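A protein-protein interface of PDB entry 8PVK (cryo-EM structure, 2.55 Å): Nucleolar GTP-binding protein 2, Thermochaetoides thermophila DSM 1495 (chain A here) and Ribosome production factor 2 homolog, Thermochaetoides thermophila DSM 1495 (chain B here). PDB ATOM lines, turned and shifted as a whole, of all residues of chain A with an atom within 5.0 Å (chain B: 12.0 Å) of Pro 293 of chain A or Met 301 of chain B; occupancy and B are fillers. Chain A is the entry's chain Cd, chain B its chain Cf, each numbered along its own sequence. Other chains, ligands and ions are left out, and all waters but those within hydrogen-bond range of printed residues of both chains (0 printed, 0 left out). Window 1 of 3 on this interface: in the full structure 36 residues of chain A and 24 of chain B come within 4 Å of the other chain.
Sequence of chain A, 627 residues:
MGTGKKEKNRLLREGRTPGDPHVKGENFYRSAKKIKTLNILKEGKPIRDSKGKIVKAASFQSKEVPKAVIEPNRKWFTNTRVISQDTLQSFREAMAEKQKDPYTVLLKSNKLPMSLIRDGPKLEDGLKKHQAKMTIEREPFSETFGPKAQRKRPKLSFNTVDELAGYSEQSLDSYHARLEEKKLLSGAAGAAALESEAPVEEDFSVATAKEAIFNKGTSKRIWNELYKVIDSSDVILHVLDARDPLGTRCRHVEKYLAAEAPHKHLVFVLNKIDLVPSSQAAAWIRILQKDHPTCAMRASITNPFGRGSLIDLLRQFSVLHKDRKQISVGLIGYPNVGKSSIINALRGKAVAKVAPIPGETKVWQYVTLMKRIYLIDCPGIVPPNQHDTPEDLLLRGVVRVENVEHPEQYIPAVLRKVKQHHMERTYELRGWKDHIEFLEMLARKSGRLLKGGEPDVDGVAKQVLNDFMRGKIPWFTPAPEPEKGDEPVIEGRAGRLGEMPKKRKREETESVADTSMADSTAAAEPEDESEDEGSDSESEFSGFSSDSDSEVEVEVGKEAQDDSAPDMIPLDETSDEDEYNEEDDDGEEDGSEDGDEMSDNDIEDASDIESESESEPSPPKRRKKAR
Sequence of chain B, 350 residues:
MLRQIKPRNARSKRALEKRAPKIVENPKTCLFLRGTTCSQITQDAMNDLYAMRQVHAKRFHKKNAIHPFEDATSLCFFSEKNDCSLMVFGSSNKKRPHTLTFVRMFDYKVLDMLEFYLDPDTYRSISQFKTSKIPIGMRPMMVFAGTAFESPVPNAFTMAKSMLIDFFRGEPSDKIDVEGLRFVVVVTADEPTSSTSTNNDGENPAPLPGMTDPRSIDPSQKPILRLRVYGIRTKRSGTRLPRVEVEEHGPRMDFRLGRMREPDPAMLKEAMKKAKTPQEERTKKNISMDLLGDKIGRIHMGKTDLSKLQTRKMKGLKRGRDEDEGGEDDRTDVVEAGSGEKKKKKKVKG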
ATOM      1  N   PRO A 102       3.054 -17.795 -20.547  1.00  0.00           N
ATOM      2  CA  PRO A 102       3.275 -17.860 -19.092  1.00  0.00           C
ATOM      3  C   PRO A 102       3.876 -16.598 -18.495  1.00  0.00           C
ATOM      4  O   PRO A 102       3.732 -16.382 -17.286  1.00  0.00           O
ATOM      5  CB  PRO A 102       4.232 -19.051 -18.931  1.00  0.00           C
ATOM      6  CG  PRO A 102       4.097 -19.832 -20.199  1.00  0.00           C
ATOM      7  CD  PRO A 102       3.822 -18.824 -21.265  1.00  0.00           C
ATOM      8  N   TYR A 103       4.530 -15.757 -19.292  1.00  0.00           N
ATOM      9  CA  TYR A 103       5.225 -14.584 -18.785  1.00  0.00           C
ATOM     10  C   TYR A 103       4.381 -13.320 -18.869  1.00  0.00           C
ATOM     11  O   TYR A 103       4.909 -12.220 -18.680  1.00  0.00           O
ATOM     12  CB  TYR A 103       6.543 -14.396 -19.535  1.00  0.00           C
ATOM     13  CG  TYR A 103       7.441 -15.606 -19.443  1.00  0.00           C
ATOM     14  CD1 TYR A 103       7.789 -16.140 -18.210  1.00  0.00           C
ATOM     15  CD2 TYR A 103       7.924 -16.225 -20.588  1.00  0.00           C
ATOM     16  CE1 TYR A 103       8.603 -17.251 -18.117  1.00  0.00           C
ATOM     17  CE2 TYR A 103       8.738 -17.336 -20.506  1.00  0.00           C
ATOM     18  CZ  TYR A 103       9.073 -17.845 -19.268  1.00  0.00           C
ATOM     19  OH  TYR A 103       9.886 -18.952 -19.181  1.00  0.00           O
ATOM     20  N   LEU A 266      -0.210 -17.142 -10.334  1.00  0.00           N
ATOM     21  CA  LEU A 266       0.334 -18.378  -9.786  1.00  0.00           C
ATOM     22  C   LEU A 266       1.787 -18.532 -10.221  1.00  0.00           C
ATOM     23  O   LEU A 266       2.087 -18.490 -11.418  1.00  0.00           O
ATOM     24  CB  LEU A 266      -0.493 -19.577 -10.247  1.00  0.00           C
ATOM     25  CG  LEU A 266      -0.075 -20.951  -9.727  1.00  0.00           C
ATOM     26  CD1 LEU A 266      -0.192 -21.010  -8.214  1.00  0.00           C
ATOM     27  CD2 LEU A 266      -0.909 -22.040 -10.377  1.00  0.00           C
ATOM     28  N   VAL A 267       2.683 -18.710  -9.252  1.00  0.00           N
ATOM     29  CA  VAL A 267       4.109 -18.880  -9.510  1.00  0.00           C
ATOM     30  C   VAL A 267       4.577 -20.159  -8.828  1.00  0.00           C
ATOM     31  O   VAL A 267       4.364 -20.340  -7.623  1.00  0.00           O
ATOM     32  CB  VAL A 267       4.922 -17.667  -9.017  1.00  0.00           C
ATOM     33  CG1 VAL A 267       6.411 -17.966  -9.045  1.00  0.00           C
ATOM     34  CG2 VAL A 267       4.612 -16.439  -9.859  1.00  0.00           C
ATOM     35  N   PHE A 268       5.208 -21.043  -9.597  1.00  0.00           N
ATOM     36  CA  PHE A 268       5.822 -22.238  -9.038  1.00  0.00           C
ATOM     37  C   PHE A 268       7.139 -21.887  -8.364  1.00  0.00           C
ATOM     38  O   PHE A 268       7.949 -21.132  -8.907  1.00  0.00           O
ATOM     39  CB  PHE A 268       6.078 -23.279 -10.128  1.00  0.00           C
ATOM     40  CG  PHE A 268       4.853 -24.014 -10.572  1.00  0.00           C
ATOM     41  CD1 PHE A 268       3.905 -24.432  -9.656  1.00  0.00           C
ATOM     42  CD2 PHE A 268       4.656 -24.300 -11.912  1.00  0.00           C
ATOM     43  CE1 PHE A 268       2.778 -25.114 -10.069  1.00  0.00           C
ATOM     44  CE2 PHE A 268       3.532 -24.980 -12.331  1.00  0.00           C
ATOM     45  CZ  PHE A 268       2.593 -25.388 -11.409  1.00  0.00           C
ATOM     46  N   ASP A 291       4.020 -24.179 -18.235  1.00  0.00           N
ATOM     47  CA  ASP A 291       2.740 -23.866 -17.610  1.00  0.00           C
ATOM     48  C   ASP A 291       2.783 -22.552 -16.839  1.00  0.00           C
ATOM     49  O   ASP A 291       1.977 -21.653 -17.094  1.00  0.00           O
ATOM     50  CB  ASP A 291       2.315 -25.009 -16.679  1.00  0.00           C
ATOM     51  CG  ASP A 291       2.006 -26.287 -17.429  1.00  0.00           C
ATOM     52  OD1 ASP A 291       1.996 -26.260 -18.677  1.00  0.00           O
ATOM     53  OD2 ASP A 291       1.769 -27.321 -16.769  1.00  0.00           O
ATOM     54  N   HIS A 292       3.708 -22.422 -15.893  1.00  0.00           N
ATOM     55  CA  HIS A 292       3.722 -21.269 -15.005  1.00  0.00           C
ATOM     56  C   HIS A 292       5.157 -20.852 -14.725  1.00  0.00           C
ATOM     57  O   HIS A 292       6.068 -21.683 -14.804  1.00  0.00           O
ATOM     58  CB  HIS A 292       2.989 -21.584 -13.690  1.00  0.00           C
ATOM     59  CG  HIS A 292       1.501 -21.661 -13.837  1.00  0.00           C
ATOM     60  ND1 HIS A 292       0.824 -22.858 -13.924  1.00  0.00           N
ATOM     61  CD2 HIS A 292       0.564 -20.689 -13.934  1.00  0.00           C
ATOM     62  CE1 HIS A 292      -0.469 -22.620 -14.056  1.00  0.00           C
ATOM     63  NE2 HIS A 292      -0.653 -21.312 -14.065  1.00  0.00           N
ATOM     64  N   PRO A 293       5.393 -19.571 -14.419  1.00  0.00           N
ATOM     65  CA  PRO A 293       6.758 -19.125 -14.096  1.00  0.00           C
ATOM     66  C   PRO A 293       7.292 -19.813 -12.848  1.00  0.00           C
ATOM     67  O   PRO A 293       6.623 -19.866 -11.815  1.00  0.00           O
ATOM     68  CB  PRO A 293       6.598 -17.617 -13.881  1.00  0.00           C
ATOM     69  CG  PRO A 293       5.340 -17.255 -14.564  1.00  0.00           C
ATOM     70  CD  PRO A 293       4.447 -18.441 -14.479  1.00  0.00           C
ATOM     71  N   THR A 294       8.518 -20.321 -12.946  1.00  0.00           N
ATOM     72  CA  THR A 294       9.105 -21.184 -11.930  1.00  0.00           C
ATOM     73  C   THR A 294      10.394 -20.570 -11.403  1.00  0.00           C
ATOM     74  O   THR A 294      11.237 -20.117 -12.184  1.00  0.00           O
ATOM     75  CB  THR A 294       9.385 -22.580 -12.497  1.00  0.00           C
ATOM     76  OG1 THR A 294       8.233 -23.048 -13.207  1.00  0.00           O
ATOM     77  CG2 THR A 294       9.713 -23.559 -11.381  1.00  0.00           C
ATOM     78  N   CYS A 295      10.540 -20.557 -10.080  1.00  0.00           N
ATOM     79  CA  CYS A 295      11.753 -20.106  -9.411  1.00  0.00           C
ATOM     80  C   CYS A 295      12.361 -21.267  -8.638  1.00  0.00           C
ATOM     81  O   CYS A 295      11.689 -21.868  -7.796  1.00  0.00           O
ATOM     82  CB  CYS A 295      11.467 -18.950  -8.447  1.00  0.00           C
ATOM     83  SG  CYS A 295      10.659 -17.512  -9.166  1.00  0.00           S
ATOM     84  N   LEU A 313      11.106 -10.971  -8.614  1.00  0.00           N
ATOM     85  CA  LEU A 313       9.797 -11.275  -9.194  1.00  0.00           C
ATOM     86  C   LEU A 313       8.664 -10.664  -8.372  1.00  0.00           C
ATOM     87  O   LEU A 313       7.707 -10.105  -8.932  1.00  0.00           O
ATOM     88  CB  LEU A 313       9.619 -12.787  -9.317  1.00  0.00           C
ATOM     89  CG  LEU A 313       8.309 -13.267  -9.944  1.00  0.00           C
ATOM     90  CD1 LEU A 313       8.154 -12.719 -11.353  1.00  0.00           C
ATOM     91  CD2 LEU A 313       8.242 -14.782  -9.945  1.00  0.00           C
ATOM     92  N   ASN B 286       5.767  -2.229 -19.117  1.00  0.00           N
ATOM     93  CA  ASN B 286       5.273  -3.590 -18.884  1.00  0.00           C
ATOM     94  C   ASN B 286       3.751  -3.664 -18.778  1.00  0.00           C
ATOM     95  O   ASN B 286       3.212  -4.660 -18.292  1.00  0.00           O
ATOM     96  CB  ASN B 286       5.919  -4.221 -17.643  1.00  0.00           C
ATOM     97  CG  ASN B 286       7.423  -4.334 -17.764  1.00  0.00           C
ATOM     98  OD1 ASN B 286       7.942  -4.825 -18.766  1.00  0.00           O
ATOM     99  ND2 ASN B 286       8.134  -3.870 -16.744  1.00  0.00           N
ATOM    100  N   ILE B 296      -2.800  -6.234 -19.563  1.00  0.00           N
ATOM    101  CA  ILE B 296      -1.840  -7.326 -19.485  1.00  0.00           C
ATOM    102  C   ILE B 296      -0.530  -6.778 -18.939  1.00  0.00           C
ATOM    103  O   ILE B 296      -0.027  -5.755 -19.422  1.00  0.00           O
ATOM    104  CB  ILE B 296      -1.632  -7.988 -20.861  1.00  0.00           C
ATOM    105  CG1 ILE B 296      -2.963  -8.504 -21.410  1.00  0.00           C
ATOM    106  CG2 ILE B 296      -0.631  -9.119 -20.771  1.00  0.00           C
ATOM    107  CD1 ILE B 296      -3.637  -9.526 -20.520  1.00  0.00           C
ATOM    108  N   GLY B 297       0.015  -7.455 -17.931  1.00  0.00           N
ATOM    109  CA  GLY B 297       1.284  -7.089 -17.333  1.00  0.00           C
ATOM    110  C   GLY B 297       2.371  -8.076 -17.715  1.00  0.00           C
ATOM    111  O   GLY B 297       2.113  -9.270 -17.875  1.00  0.00           O
ATOM    112  N   ARG B 298       3.591  -7.568 -17.853  1.00  0.00           N
ATOM    113  CA  ARG B 298       4.742  -8.359 -18.264  1.00  0.00           C
ATOM    114  C   ARG B 298       5.660  -8.605 -17.075  1.00  0.00           C
ATOM    115  O   ARG B 298       5.954  -7.686 -16.305  1.00  0.00           O
ATOM    116  CB  ARG B 298       5.521  -7.653 -19.377  1.00  0.00           C
ATOM    117  CG  ARG B 298       5.249  -8.174 -20.775  1.00  0.00           C
ATOM    118  CD  ARG B 298       6.049  -9.430 -21.074  1.00  0.00           C
ATOM    119  NE  ARG B 298       5.707  -9.982 -22.381  1.00  0.00           N
ATOM    120  CZ  ARG B 298       6.002 -11.212 -22.776  1.00  0.00           C
ATOM    121  NH1 ARG B 298       6.652 -12.055 -21.991  1.00  0.00           N
ATOM    122  NH2 ARG B 298       5.631 -11.610 -23.989  1.00  0.00           N
ATOM    123  N   ILE B 299       6.112  -9.848 -16.931  1.00  0.00           N
ATOM    124  CA  ILE B 299       7.093 -10.208 -15.919  1.00  0.00           C
ATOM    125  C   ILE B 299       8.313 -10.787 -16.620  1.00  0.00           C
ATOM    126  O   ILE B 299       8.234 -11.304 -17.737  1.00  0.00           O
ATOM    127  CB  ILE B 299       6.535 -11.200 -14.877  1.00  0.00           C
ATOM    128  CG1 ILE B 299       6.039 -12.474 -15.560  1.00  0.00           C
ATOM    129  CG2 ILE B 299       5.423 -10.554 -14.068  1.00  0.00           C
ATOM    130  CD1 ILE B 299       5.647 -13.559 -14.595  1.00  0.00           C
ATOM    131  N   HIS B 300       9.458 -10.686 -15.949  1.00  0.00           N
ATOM    132  CA  HIS B 300      10.744 -11.050 -16.534  1.00  0.00           C
ATOM    133  C   HIS B 300      11.504 -11.917 -15.542  1.00  0.00           C
ATOM    134  O   HIS B 300      11.953 -11.429 -14.500  1.00  0.00           O
ATOM    135  CB  HIS B 300      11.542  -9.802 -16.906  1.00  0.00           C
ATOM    136  CG  HIS B 300      10.768  -8.829 -17.737  1.00  0.00           C
ATOM    137  ND1 HIS B 300      10.626  -8.962 -19.101  1.00  0.00           N
ATOM    138  CD2 HIS B 300      10.074  -7.719 -17.393  1.00  0.00           C
ATOM    139  CE1 HIS B 300       9.887  -7.970 -19.563  1.00  0.00           C
ATOM    140  NE2 HIS B 300       9.540  -7.201 -18.547  1.00  0.00           N
ATOM    141  N   MET B 301      11.648 -13.200 -15.870  1.00  0.00           N
ATOM    142  CA  MET B 301      12.262 -14.151 -14.950  1.00  0.00           C
ATOM    143  C   MET B 301      13.783 -14.080 -14.986  1.00  0.00           C
ATOM    144  O   MET B 301      14.432 -14.118 -13.935  1.00  0.00           O
ATOM    145  CB  MET B 301      11.789 -15.567 -15.280  1.00  0.00           C
ATOM    146  CG  MET B 301      10.281 -15.733 -15.227  1.00  0.00           C
ATOM    147  SD  MET B 301       9.631 -15.613 -13.555  1.00  0.00           S
ATOM    148  CE  MET B 301      10.797 -16.648 -12.677  1.00  0.00           C
ATOM    149  N   GLY B 302      14.366 -13.978 -16.175  1.00  0.00           N
ATOM    150  CA  GLY B 302      15.802 -14.020 -16.326  1.00  0.00           C
ATOM    151  C   GLY B 302      16.321 -15.436 -16.497  1.00  0.00           C
ATOM    152  O   GLY B 302      15.605 -16.428 -16.339  1.00  0.00           O
ATOM    153  N   LYS B 303      17.604 -15.523 -16.837  1.00  0.00           N
ATOM    154  CA  LYS B 303      18.232 -16.816 -17.061  1.00  0.00           C
ATOM    155  C   LYS B 303      18.441 -17.550 -15.742  1.00  0.00           C
ATOM    156  O   LYS B 303      18.862 -16.961 -14.743  1.00  0.00           O
ATOM    157  CB  LYS B 303      19.568 -16.638 -17.780  1.00  0.00           C
ATOM    158  N   THR B 304      18.142 -18.847 -15.746  1.00  0.00           N
ATOM    159  CA  THR B 304      18.314 -19.692 -14.570  1.00  0.00           C
ATOM    160  C   THR B 304      19.746 -20.214 -14.557  1.00  0.00           C
ATOM    161  O   THR B 304      20.131 -21.017 -15.413  1.00  0.00           O
ATOM    162  CB  THR B 304      17.312 -20.843 -14.576  1.00  0.00           C
ATOM    163  N   ASP B 305      20.533 -19.760 -13.585  1.00  0.00           N
ATOM    164  CA  ASP B 305      21.942 -20.128 -13.463  1.00  0.00           C
ATOM    165  C   ASP B 305      22.112 -20.941 -12.185  1.00  0.00           C
ATOM    166  O   ASP B 305      22.224 -20.378 -11.091  1.00  0.00           O
ATOM    167  CB  ASP B 305      22.834 -18.889 -13.459  1.00  0.00           C
ATOM    168  N   LEU B 306      22.134 -22.264 -12.326  1.00  0.00           N
ATOM    169  CA  LEU B 306      22.315 -23.172 -11.203  1.00  0.00           C
ATOM    170  C   LEU B 306      23.759 -23.630 -11.052  1.00  0.00           C
ATOM    171  O   LEU B 306      24.025 -24.559 -10.284  1.00  0.00           O
ATOM    172  CB  LEU B 306      21.394 -24.386 -11.349  1.00  0.00           C
ATOM    173  CG  LEU B 306      19.981 -24.271 -10.773  1.00  0.00           C
ATOM    174  CD1 LEU B 306      19.066 -23.469 -11.684  1.00  0.00           C
ATOM    175  CD2 LEU B 306      19.404 -25.649 -10.517  1.00  0.00           C
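No residue of chain B comes within 4 Å of Pro 102 of chain A. Tyr 103 of chain A touches three residues of chain B. Pro 293 of chain A touches just these residues of chain B: Ile 299 (3.7 Å) and Met 301 (3.6 Å). Thr 294 of chain A touches just one residue of chain B: Met 301 (3.5 Å). Cys 295 of chain A touches just one residue of chain B: Met 301 (3.6 Å). Of chain B, only Met 301 (3.9 Å) comes within 4 Å of Leu 313 of chain A. Of the printed residues of chain A, Arg 298 of chain B touches Tyr 103. Printed residues of chain A within 4 Å of Ile 299 of chain B: Tyr 103 (3.2 Å) and Pro 293 (3.7 Å). Of chain A, only Tyr 103, Pro 293, Thr 294, Cys 295 and Leu 313 come within 4 Å of Met 301 of chain B. Leu 306 of chain B touches none of the printed residues of chain A. The nearest printed residue of chain A that does not touch Arg 298 of chain B is Pro 102 of chain A (6.4 Å).
Among the printed residues, merely in contact across the chains: Tyr 103 of chain A with Arg 298 of chain B (3.4 Å), Tyr 103 of chain A with Met 301 of chain B (3.7 Å), Pro 293 of chain A with Ile 299 of chain B (3.7 Å), Pro 293 of chain A with Met 301 of chain B (3.6 Å), Thr 294 of chain A with Met 301 of chain B (3.5 Å), Cys 295 of chain A with Met 301 of chain B (3.6 Å) and Leu 313 of chain A with Met 301 of chain B (3.9 Å).
N of Ile 299 of chain B lies within hydrogen-bond range of O of Tyr 103 of chain A.
Of the 11 printed residues of chain A, 5 touch a printed residue of chain B. Among the printed residues, 8 pairs touch across the chains.
N of Phe 268 of chain A is in hydrogen-bond range of O of Pro 293 of chain A (2.9 Å). O of Phe 268 of chain A sits at hydrogen-bond distance from N of Cys 295 of chain A, at 2.9 Å. The side-chain hydroxyl (OG1) of Thr 294 of chain A is in hydrogen-bond range of the backbone carbonyl oxygen (O) of His 292 of chain A (3.0 Å). The backbone NH of Arg 298 of chain B is in hydrogen-bond range of the backbone carbonyl oxygen of Asn 286 of chain B, 3.0 Å away.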
